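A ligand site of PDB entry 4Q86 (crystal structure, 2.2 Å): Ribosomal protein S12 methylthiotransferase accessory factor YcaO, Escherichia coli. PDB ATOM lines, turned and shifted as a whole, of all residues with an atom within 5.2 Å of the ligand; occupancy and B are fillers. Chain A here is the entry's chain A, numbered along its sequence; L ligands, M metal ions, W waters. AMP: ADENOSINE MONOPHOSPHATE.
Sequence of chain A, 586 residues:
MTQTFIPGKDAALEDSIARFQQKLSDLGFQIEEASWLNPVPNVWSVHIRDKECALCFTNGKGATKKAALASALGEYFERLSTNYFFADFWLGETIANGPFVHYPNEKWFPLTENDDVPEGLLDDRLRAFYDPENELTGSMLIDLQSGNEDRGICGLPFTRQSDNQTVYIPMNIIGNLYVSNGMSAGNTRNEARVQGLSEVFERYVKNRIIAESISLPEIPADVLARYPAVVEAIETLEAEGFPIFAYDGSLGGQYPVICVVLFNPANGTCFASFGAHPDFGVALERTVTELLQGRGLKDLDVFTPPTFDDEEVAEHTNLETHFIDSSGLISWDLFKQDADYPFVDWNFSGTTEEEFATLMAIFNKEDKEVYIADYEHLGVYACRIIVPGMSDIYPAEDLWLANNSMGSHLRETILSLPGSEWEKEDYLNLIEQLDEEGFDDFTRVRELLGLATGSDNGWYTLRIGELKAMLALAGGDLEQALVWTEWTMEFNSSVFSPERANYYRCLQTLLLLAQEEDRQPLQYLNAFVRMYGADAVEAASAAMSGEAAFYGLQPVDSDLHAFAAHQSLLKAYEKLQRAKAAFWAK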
ATOM      1  N   LYS A   9     -19.454 -14.668  -5.008  1.00  0.00           N
ATOM      2  CA  LYS A   9     -18.780 -13.801  -4.050  1.00  0.00           C
ATOM      3  C   LYS A   9     -18.504 -14.470  -2.702  1.00  0.00           C
ATOM      4  O   LYS A   9     -19.365 -15.142  -2.135  1.00  0.00           O
ATOM      5  CB  LYS A   9     -19.621 -12.552  -3.804  1.00  0.00           C
ATOM      6  CG  LYS A   9     -19.952 -11.809  -5.088  1.00  0.00           C
ATOM      7  CD  LYS A   9     -18.695 -11.295  -5.803  1.00  0.00           C
ATOM      8  CE  LYS A   9     -19.009 -10.354  -6.961  1.00  0.00           C
ATOM      9  NZ  LYS A   9     -17.821 -10.209  -7.829  1.00  0.00           N
ATOM     10  N   LEU A  13     -22.670  -8.729   0.525  1.00  0.00           N
ATOM     11  CA  LEU A  13     -22.626  -7.412  -0.085  1.00  0.00           C
ATOM     12  C   LEU A  13     -22.417  -6.307   0.943  1.00  0.00           C
ATOM     13  O   LEU A  13     -21.579  -5.435   0.740  1.00  0.00           O
ATOM     14  CB  LEU A  13     -23.883  -7.109  -0.899  1.00  0.00           C
ATOM     15  CG  LEU A  13     -24.156  -8.018  -2.097  1.00  0.00           C
ATOM     16  CD1 LEU A  13     -25.425  -7.588  -2.812  1.00  0.00           C
ATOM     17  CD2 LEU A  13     -22.999  -8.026  -3.075  1.00  0.00           C
ATOM     18  N   SER A  16     -18.776  -6.232   2.354  1.00  0.00           N
ATOM     19  CA  SER A  16     -17.889  -5.629   1.358  1.00  0.00           C
ATOM     20  C   SER A  16     -18.047  -4.096   1.316  1.00  0.00           C
ATOM     21  O   SER A  16     -17.049  -3.360   1.279  1.00  0.00           O
ATOM     22  CB  SER A  16     -18.166  -6.191  -0.047  1.00  0.00           C
ATOM     23  OG  SER A  16     -18.165  -7.606  -0.057  1.00  0.00           O
ATOM     24  N   PHE A  20     -15.102  -1.622   2.353  1.00  0.00           N
ATOM     25  CA  PHE A  20     -14.464  -0.792   1.319  1.00  0.00           C
ATOM     26  C   PHE A  20     -14.628   0.687   1.621  1.00  0.00           C
ATOM     27  O   PHE A  20     -13.695   1.454   1.461  1.00  0.00           O
ATOM     28  CB  PHE A  20     -15.039  -1.096  -0.040  1.00  0.00           C
ATOM     29  CG  PHE A  20     -14.706  -2.462  -0.587  1.00  0.00           C
ATOM     30  CD1 PHE A  20     -13.704  -3.242  -0.023  1.00  0.00           C
ATOM     31  CD2 PHE A  20     -15.392  -2.952  -1.681  1.00  0.00           C
ATOM     32  CE1 PHE A  20     -13.431  -4.510  -0.540  1.00  0.00           C
ATOM     33  CE2 PHE A  20     -15.118  -4.201  -2.211  1.00  0.00           C
ATOM     34  CZ  PHE A  20     -14.134  -4.978  -1.633  1.00  0.00           C
ATOM     35  N   ASN A  59     -17.464   3.195 -12.074  1.00  0.00           N
ATOM     36  CA  ASN A  59     -18.865   2.870 -12.173  1.00  0.00           C
ATOM     37  C   ASN A  59     -19.162   1.435 -11.700  1.00  0.00           C
ATOM     38  O   ASN A  59     -18.322   0.534 -11.826  1.00  0.00           O
ATOM     39  CB  ASN A  59     -19.326   3.019 -13.606  1.00  0.00           C
ATOM     40  CG  ASN A  59     -19.195   4.453 -14.111  1.00  0.00           C
ATOM     41  OD1 ASN A  59     -19.891   5.343 -13.664  1.00  0.00           O
ATOM     42  ND2 ASN A  59     -18.268   4.667 -15.013  1.00  0.00           N
ATOM     43  N   GLY A  60     -20.332   1.288 -11.100  1.00  0.00           N
ATOM     44  CA  GLY A  60     -20.766   0.042 -10.560  1.00  0.00           C
ATOM     45  C   GLY A  60     -21.894  -0.485 -11.385  1.00  0.00           C
ATOM     46  O   GLY A  60     -22.576   0.258 -12.081  1.00  0.00           O
ATOM     47  N   LYS A  61     -22.073  -1.801 -11.323  1.00  0.00           N
ATOM     48  CA  LYS A  61     -23.188  -2.447 -11.970  1.00  0.00           C
ATOM     49  C   LYS A  61     -23.560  -3.707 -11.179  1.00  0.00           C
ATOM     50  O   LYS A  61     -22.744  -4.310 -10.502  1.00  0.00           O
ATOM     51  CB  LYS A  61     -22.845  -2.825 -13.411  1.00  0.00           C
ATOM     52  CG  LYS A  61     -21.817  -3.938 -13.538  1.00  0.00           C
ATOM     53  CD  LYS A  61     -21.467  -4.311 -14.964  1.00  0.00           C
ATOM     54  CE  LYS A  61     -20.197  -5.149 -14.975  1.00  0.00           C
ATOM     55  NZ  LYS A  61     -20.204  -6.160 -16.056  1.00  0.00           N
ATOM     56  N   ALA A  67     -25.430  -4.613  -4.805  1.00  0.00           N
ATOM     57  CA  ALA A  67     -24.464  -5.268  -5.683  1.00  0.00           C
ATOM     58  C   ALA A  67     -23.766  -4.243  -6.588  1.00  0.00           C
ATOM     59  O   ALA A  67     -22.574  -4.346  -6.810  1.00  0.00           O
ATOM     60  CB  ALA A  67     -25.126  -6.355  -6.518  1.00  0.00           C
ATOM     61  N   ALA A  70     -21.253  -2.252  -4.393  1.00  0.00           N
ATOM     62  CA  ALA A  70     -20.068  -3.061  -4.088  1.00  0.00           C
ATOM     63  C   ALA A  70     -19.160  -3.174  -5.322  1.00  0.00           C
ATOM     64  O   ALA A  70     -17.930  -3.146  -5.215  1.00  0.00           O
ATOM     65  CB  ALA A  70     -20.497  -4.449  -3.599  1.00  0.00           C
ATOM     66  N   SER A  71     -19.794  -3.308  -6.491  1.00  0.00           N
ATOM     67  CA  SER A  71     -19.079  -3.277  -7.764  1.00  0.00           C
ATOM     68  C   SER A  71     -18.312  -1.969  -8.003  1.00  0.00           C
ATOM     69  O   SER A  71     -17.152  -1.978  -8.399  1.00  0.00           O
ATOM     70  CB  SER A  71     -20.079  -3.523  -8.899  1.00  0.00           C
ATOM     71  OG  SER A  71     -19.601  -3.055 -10.126  1.00  0.00           O
ATOM     72  N   GLY A  74     -15.459  -1.848  -5.468  1.00  0.00           N
ATOM     73  CA  GLY A  74     -14.459  -2.844  -5.852  1.00  0.00           C
ATOM     74  C   GLY A  74     -13.608  -2.334  -7.004  1.00  0.00           C
ATOM     75  O   GLY A  74     -12.387  -2.488  -6.986  1.00  0.00           O
ATOM     76  N   GLU A  75     -14.270  -1.747  -8.013  1.00  0.00           N
ATOM     77  CA  GLU A  75     -13.568  -1.214  -9.159  1.00  0.00           C
ATOM     78  C   GLU A  75     -12.688  -0.054  -8.717  1.00  0.00           C
ATOM     79  O   GLU A  75     -11.580   0.106  -9.213  1.00  0.00           O
ATOM     80  CB  GLU A  75     -14.514  -0.743 -10.270  1.00  0.00           C
ATOM     81  CG  GLU A  75     -13.830  -0.600 -11.631  1.00  0.00           C
ATOM     82  CD  GLU A  75     -14.819  -0.404 -12.775  1.00  0.00           C
ATOM     83  OE1 GLU A  75     -15.042  -1.310 -13.628  1.00  0.00           O
ATOM     84  OE2 GLU A  75     -15.405   0.699 -12.798  1.00  0.00           O
ATOM     85  N   GLU A  78      -9.625  -1.654  -7.326  1.00  0.00           N
ATOM     86  CA  GLU A  78      -8.894  -2.209  -8.482  1.00  0.00           C
ATOM     87  C   GLU A  78      -8.061  -1.137  -9.199  1.00  0.00           C
ATOM     88  O   GLU A  78      -6.881  -1.342  -9.484  1.00  0.00           O
ATOM     89  CB  GLU A  78      -9.919  -2.862  -9.401  1.00  0.00           C
ATOM     90  CG  GLU A  78      -9.523  -3.039 -10.834  1.00  0.00           C
ATOM     91  CD  GLU A  78     -10.714  -3.453 -11.699  1.00  0.00           C
ATOM     92  OE1 GLU A  78     -11.461  -4.398 -11.296  1.00  0.00           O
ATOM     93  OE2 GLU A  78     -10.856  -2.913 -12.805  1.00  0.00           O
ATOM     94  N   MET A 183      -7.421  -6.521 -14.699  1.00  0.00           N
ATOM     95  CA  MET A 183      -7.274  -6.048 -13.321  1.00  0.00           C
ATOM     96  C   MET A 183      -8.492  -6.530 -12.602  1.00  0.00           C
ATOM     97  O   MET A 183      -9.491  -6.832 -13.214  1.00  0.00           O
ATOM     98  CB  MET A 183      -7.332  -4.535 -13.181  1.00  0.00           C
ATOM     99  CG  MET A 183      -6.649  -3.742 -14.228  1.00  0.00           C
ATOM    100  SD  MET A 183      -6.648  -2.007 -13.794  1.00  0.00           S
ATOM    101  CE  MET A 183      -5.034  -1.738 -14.494  1.00  0.00           C
ATOM    102  N   SER A 184      -8.398  -6.569 -11.278  1.00  0.00           N
ATOM    103  CA  SER A 184      -9.477  -6.983 -10.440  1.00  0.00           C
ATOM    104  C   SER A 184      -9.149  -6.645  -8.981  1.00  0.00           C
ATOM    105  O   SER A 184      -8.012  -6.540  -8.612  1.00  0.00           O
ATOM    106  CB  SER A 184      -9.707  -8.523 -10.607  1.00  0.00           C
ATOM    107  OG  SER A 184     -10.816  -8.924  -9.827  1.00  0.00           O
ATOM    108  N   ALA A 185     -10.191  -6.485  -8.186  1.00  0.00           N
ATOM    109  CA  ALA A 185     -10.129  -6.487  -6.727  1.00  0.00           C
ATOM    110  C   ALA A 185     -11.248  -7.428  -6.177  1.00  0.00           C
ATOM    111  O   ALA A 185     -12.160  -7.804  -6.902  1.00  0.00           O
ATOM    112  CB  ALA A 185     -10.301  -5.079  -6.181  1.00  0.00           C
ATOM    113  N   GLY A 186     -11.167  -7.744  -4.892  1.00  0.00           N
ATOM    114  CA  GLY A 186     -12.136  -8.616  -4.328  1.00  0.00           C
ATOM    115  C   GLY A 186     -12.077  -8.777  -2.829  1.00  0.00           C
ATOM    116  O   GLY A 186     -11.189  -8.255  -2.155  1.00  0.00           O
ATOM    117  N   ASN A 187     -13.066  -9.491  -2.322  1.00  0.00           N
ATOM    118  CA  ASN A 187     -13.128  -9.826  -0.898  1.00  0.00           C
ATOM    119  C   ASN A 187     -12.015 -10.779  -0.514  1.00  0.00           C
ATOM    120  O   ASN A 187     -11.560 -10.774   0.636  1.00  0.00           O
ATOM    121  CB  ASN A 187     -14.468 -10.471  -0.572  1.00  0.00           C
ATOM    122  CG  ASN A 187     -15.620  -9.578  -0.855  1.00  0.00           C
ATOM    123  OD1 ASN A 187     -15.745  -8.500  -0.269  1.00  0.00           O
ATOM    124  ND2 ASN A 187     -16.492  -9.994  -1.764  1.00  0.00           N
ATOM    125  N   GLU A 191     -11.467 -14.929  -5.246  1.00  0.00           N
ATOM    126  CA  GLU A 191     -12.645 -14.250  -5.820  1.00  0.00           C
ATOM    127  C   GLU A 191     -12.201 -13.186  -6.845  1.00  0.00           C
ATOM    128  O   GLU A 191     -12.710 -13.144  -7.982  1.00  0.00           O
ATOM    129  CB  GLU A 191     -13.502 -13.598  -4.722  1.00  0.00           C
ATOM    130  CG  GLU A 191     -14.719 -12.804  -5.207  1.00  0.00           C
ATOM    131  CD  GLU A 191     -15.174 -11.763  -4.189  1.00  0.00           C
ATOM    132  OE1 GLU A 191     -15.816 -12.117  -3.157  1.00  0.00           O
ATOM    133  OE2 GLU A 191     -14.803 -10.581  -4.375  1.00  0.00           O
ATOM    134  N   ALA A 192     -11.183 -12.390  -6.459  1.00  0.00           N
ATOM    135  CA  ALA A 192     -10.618 -11.383  -7.330  1.00  0.00           C
ATOM    136  C   ALA A 192     -10.015 -12.025  -8.557  1.00  0.00           C
ATOM    137  O   ALA A 192     -10.198 -11.527  -9.690  1.00  0.00           O
ATOM    138  CB  ALA A 192      -9.573 -10.557  -6.578  1.00  0.00           C
ATOM    139  N   GLN A 195     -12.490 -13.312 -11.072  1.00  0.00           N
ATOM    140  CA  GLN A 195     -13.053 -12.185 -11.844  1.00  0.00           C
ATOM    141  C   GLN A 195     -12.074 -11.725 -12.941  1.00  0.00           C
ATOM    142  O   GLN A 195     -12.464 -11.528 -14.076  1.00  0.00           O
ATOM    143  CB  GLN A 195     -13.482 -11.039 -10.897  1.00  0.00           C
ATOM    144  CG  GLN A 195     -14.476 -10.041 -11.512  1.00  0.00           C
ATOM    145  CD  GLN A 195     -13.824  -9.009 -12.412  1.00  0.00           C
ATOM    146  OE1 GLN A 195     -14.350  -8.676 -13.455  1.00  0.00           O
ATOM    147  NE2 GLN A 195     -12.649  -8.540 -12.049  1.00  0.00           N
ATOM    148  N   ARG A 286     -24.018 -10.495 -15.672  1.00  0.00           N
ATOM    149  CA  ARG A 286     -22.979  -9.466 -15.930  1.00  0.00           C
ATOM    150  C   ARG A 286     -23.150  -8.874 -17.291  1.00  0.00           C
ATOM    151  O   ARG A 286     -22.801  -7.729 -17.480  1.00  0.00           O
ATOM    152  CB  ARG A 286     -21.595 -10.044 -16.090  1.00  0.00           C
ATOM    153  CG  ARG A 286     -20.940 -10.527 -14.848  1.00  0.00           C
ATOM    154  CD  ARG A 286     -19.525 -10.968 -15.140  1.00  0.00           C
ATOM    155  NE  ARG A 286     -18.631  -9.866 -15.453  1.00  0.00           N
ATOM    156  CZ  ARG A 286     -18.402  -8.817 -14.669  1.00  0.00           C
ATOM    157  NH1 ARG A 286     -18.995  -8.681 -13.513  1.00  0.00           N
ATOM    158  NH2 ARG A 286     -17.543  -7.900 -15.045  1.00  0.00           N
ATOM    159  N   GLN A 293     -25.153  -0.305 -18.052  1.00  0.00           N
ATOM    160  CA  GLN A 293     -24.373   0.503 -17.133  1.00  0.00           C
ATOM    161  C   GLN A 293     -24.270   1.960 -17.547  1.00  0.00           C
ATOM    162  O   GLN A 293     -23.733   2.301 -18.601  1.00  0.00           O
ATOM    163  CB  GLN A 293     -22.943  -0.030 -16.982  1.00  0.00           C
ATOM    164  CG  GLN A 293     -22.181   0.818 -15.963  1.00  0.00           C
ATOM    165  CD  GLN A 293     -20.899   0.207 -15.548  1.00  0.00           C
ATOM    166  OE1 GLN A 293     -20.717  -0.199 -14.382  1.00  0.00           O
ATOM    167  NE2 GLN A 293     -19.990   0.103 -16.505  1.00  0.00           N
HETATM  168  P   AMP L   1     -17.798  -5.518 -11.971  1.00  0.00           P
HETATM  169  O1P AMP L   1     -18.700  -6.691 -11.641  1.00  0.00           O
HETATM  170  O2P AMP L   1     -18.531  -4.214 -12.056  1.00  0.00           O
HETATM  171  O3P AMP L   1     -16.873  -5.819 -13.130  1.00  0.00           O
HETATM  172  O5' AMP L   1     -16.861  -5.327 -10.674  1.00  0.00           O
HETATM  173  C5' AMP L   1     -15.823  -4.382 -10.647  1.00  0.00           C
HETATM  174  C4' AMP L   1     -14.846  -4.790  -9.573  1.00  0.00           C
HETATM  175  O4' AMP L   1     -15.535  -5.148  -8.331  1.00  0.00           O
HETATM  176  C3' AMP L   1     -14.058  -6.036  -9.957  1.00  0.00           C
HETATM  177  O3' AMP L   1     -12.665  -5.892  -9.719  1.00  0.00           O
HETATM  178  C2' AMP L   1     -14.623  -7.071  -8.994  1.00  0.00           C
HETATM  179  O2' AMP L   1     -13.741  -8.167  -8.981  1.00  0.00           O
HETATM  180  C1' AMP L   1     -14.800  -6.223  -7.729  1.00  0.00           C
HETATM  181  N9  AMP L   1     -15.506  -6.660  -6.443  1.00  0.00           N
HETATM  182  C8  AMP L   1     -15.064  -6.833  -5.134  1.00  0.00           C
HETATM  183  N7  AMP L   1     -16.057  -7.184  -4.251  1.00  0.00           N
HETATM  184  C5  AMP L   1     -17.119  -7.133  -5.060  1.00  0.00           C
HETATM  185  C6  AMP L   1     -18.489  -7.370  -4.918  1.00  0.00           C
HETATM  186  N6  AMP L   1     -19.048  -7.703  -3.731  1.00  0.00           N
HETATM  187  N1  AMP L   1     -19.166  -7.200  -6.079  1.00  0.00           N
HETATM  188  C2  AMP L   1     -18.721  -6.879  -7.325  1.00  0.00           C
HETATM  189  N3  AMP L   1     -17.483  -6.678  -7.533  1.00  0.00           N
HETATM  190  C4  AMP L   1     -16.753  -6.776  -6.443  1.00  0.00           C
HETATM  191 MG    MG M   1     -16.793  -1.681 -15.058  1.00  0.00          MG
HETATM  192 MG    MG M   2     -13.016  -5.144 -14.992  1.00  0.00          MG
HETATM  193  O   HOH W   1     -21.440  -6.758  -6.871  1.00  0.00           O
HETATM  194  O   HOH W   2     -19.902  -8.975  -1.444  1.00  0.00           O
HETATM  195  O   HOH W   3     -17.771  -9.042 -10.434  1.00  0.00           O
HETATM  196  O   HOH W   4     -14.635  -6.077 -14.459  1.00  0.00           O
HETATM  197  O   HOH W   5     -21.366  -6.380 -11.088  1.00  0.00           O
HETATM  198  O   HOH W   6     -17.840  -1.889 -13.227  1.00  0.00           O
HETATM  199  O   HOH W   7     -15.138  -9.677  -7.076  1.00  0.00           O
HETATM  200  O   HOH W   8     -16.957  -3.777 -14.600  1.00  0.00           O
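Lys 9 touches the ligand. Ser 16 touches the ligand (OG to N6, 3.8 Å). CE2 of Phe 20 touches N7 of the ligand, 3.7 Å away. Lys 61 touches the ligand. Ala 70 touches the ligand (CB to N6, 3.6 Å). CA of Gly 74 touches O4' of the ligand, at 3.6 Å. Glu 75 touches the ligand (N to C4', 3.5 Å). Gly 186 touches the ligand. ND2 of Asn 187 touches N7 of the ligand, at 3.8 Å. Glu 191 touches the ligand (OE2 to N7, 3.6 Å). Hydrophobic or aromatic side chains that line the ligand: Phe 20 and Ala 70. Within 4 Å of the ligand: Lys 9, Ser 16, Phe 20, Lys 61, Ala 70, Ser 71, Gly 74, Glu 75, Glu 78, Ser 184, Ala 185, Gly 186, Asn 187, Glu 191, Gln 195 and Arg 286. Along chain A the residues within 4 Å of the ligand span positions 9 to 286.
Water W4 lies within hydrogen-bond range of O3P of the ligand (2.6 Å), OE1 of Gln 195 (2.8 Å) and NH2 of Arg 286 (3.5 Å). Water W6 bridges O2P of the ligand (2.7 Å) and O of Asn 59 (2.8 Å). Water W5 lies within hydrogen-bond range of O of Lys 61 (2.6 Å) and O1P of the ligand (2.7 Å). Water W2 lies within hydrogen-bond range of the side-chain hydroxyl of Ser 16, a nitrogen (N6) of the ligand and the backbone NH of Leu 13. Water W3 lies within hydrogen-bond range of O1P of the ligand (2.8 Å), NZ of Lys 9 (2.9 Å) and NH1 of Arg 286 (3.3 Å). Water W7 lies within hydrogen-bond range of an oxygen (O2') of the ligand (2.8 Å), the side-chain amino group of Lys 9 (2.8 Å) and the side-chain carboxylate of Glu 191 (2.9 Å).
The side-chain carboxylate (OE1) of Glu 78 sits at hydrogen-bond distance from an oxygen (O3') of the ligand (2.5 Å). The side-chain hydroxyl of Ser 71 lies within hydrogen-bond range of an oxygen (O2P) of the ligand (2.5 Å). N of Ala 185 is in hydrogen-bond range of O3' of the ligand (3.0 Å). An oxygen (O2') of the ligand is in hydrogen-bond range of the backbone carbonyl oxygen (O) of Ala 185. O1P of the ligand lies within salt-bridge range of NH1 of Arg 286. O2' of the ligand is in hydrogen-bond range of OG of Ser 184 (3.1 Å). NE2 of Gln 195 lies close to O2' of the ligand, 3.3 Å away.
N of Lys 61 lies within hydrogen-bond range of OG of Ser 71, at 3.0 Å. The backbone carbonyl oxygen of Arg 286 is in hydrogen-bond range of the side-chain amino group of Lys 61. The side-chain hydroxyl of Ser 184 lies within hydrogen-bond range of the side-chain amide nitrogen of Gln 195. OG of Ser 184 sits at hydrogen-bond distance from O of Ala 192 (2.7 Å). The backbone NH of Asn 59 sits at hydrogen-bond distance from the side-chain carboxylate of Glu 75, 3.3 Å away. ND2 of Asn 187 sits at hydrogen-bond distance from OE1 of Glu 191 (2.6 Å). OG of Ser 16 lies within hydrogen-bond range of OD1 of Asn 187, at 2.6 Å.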
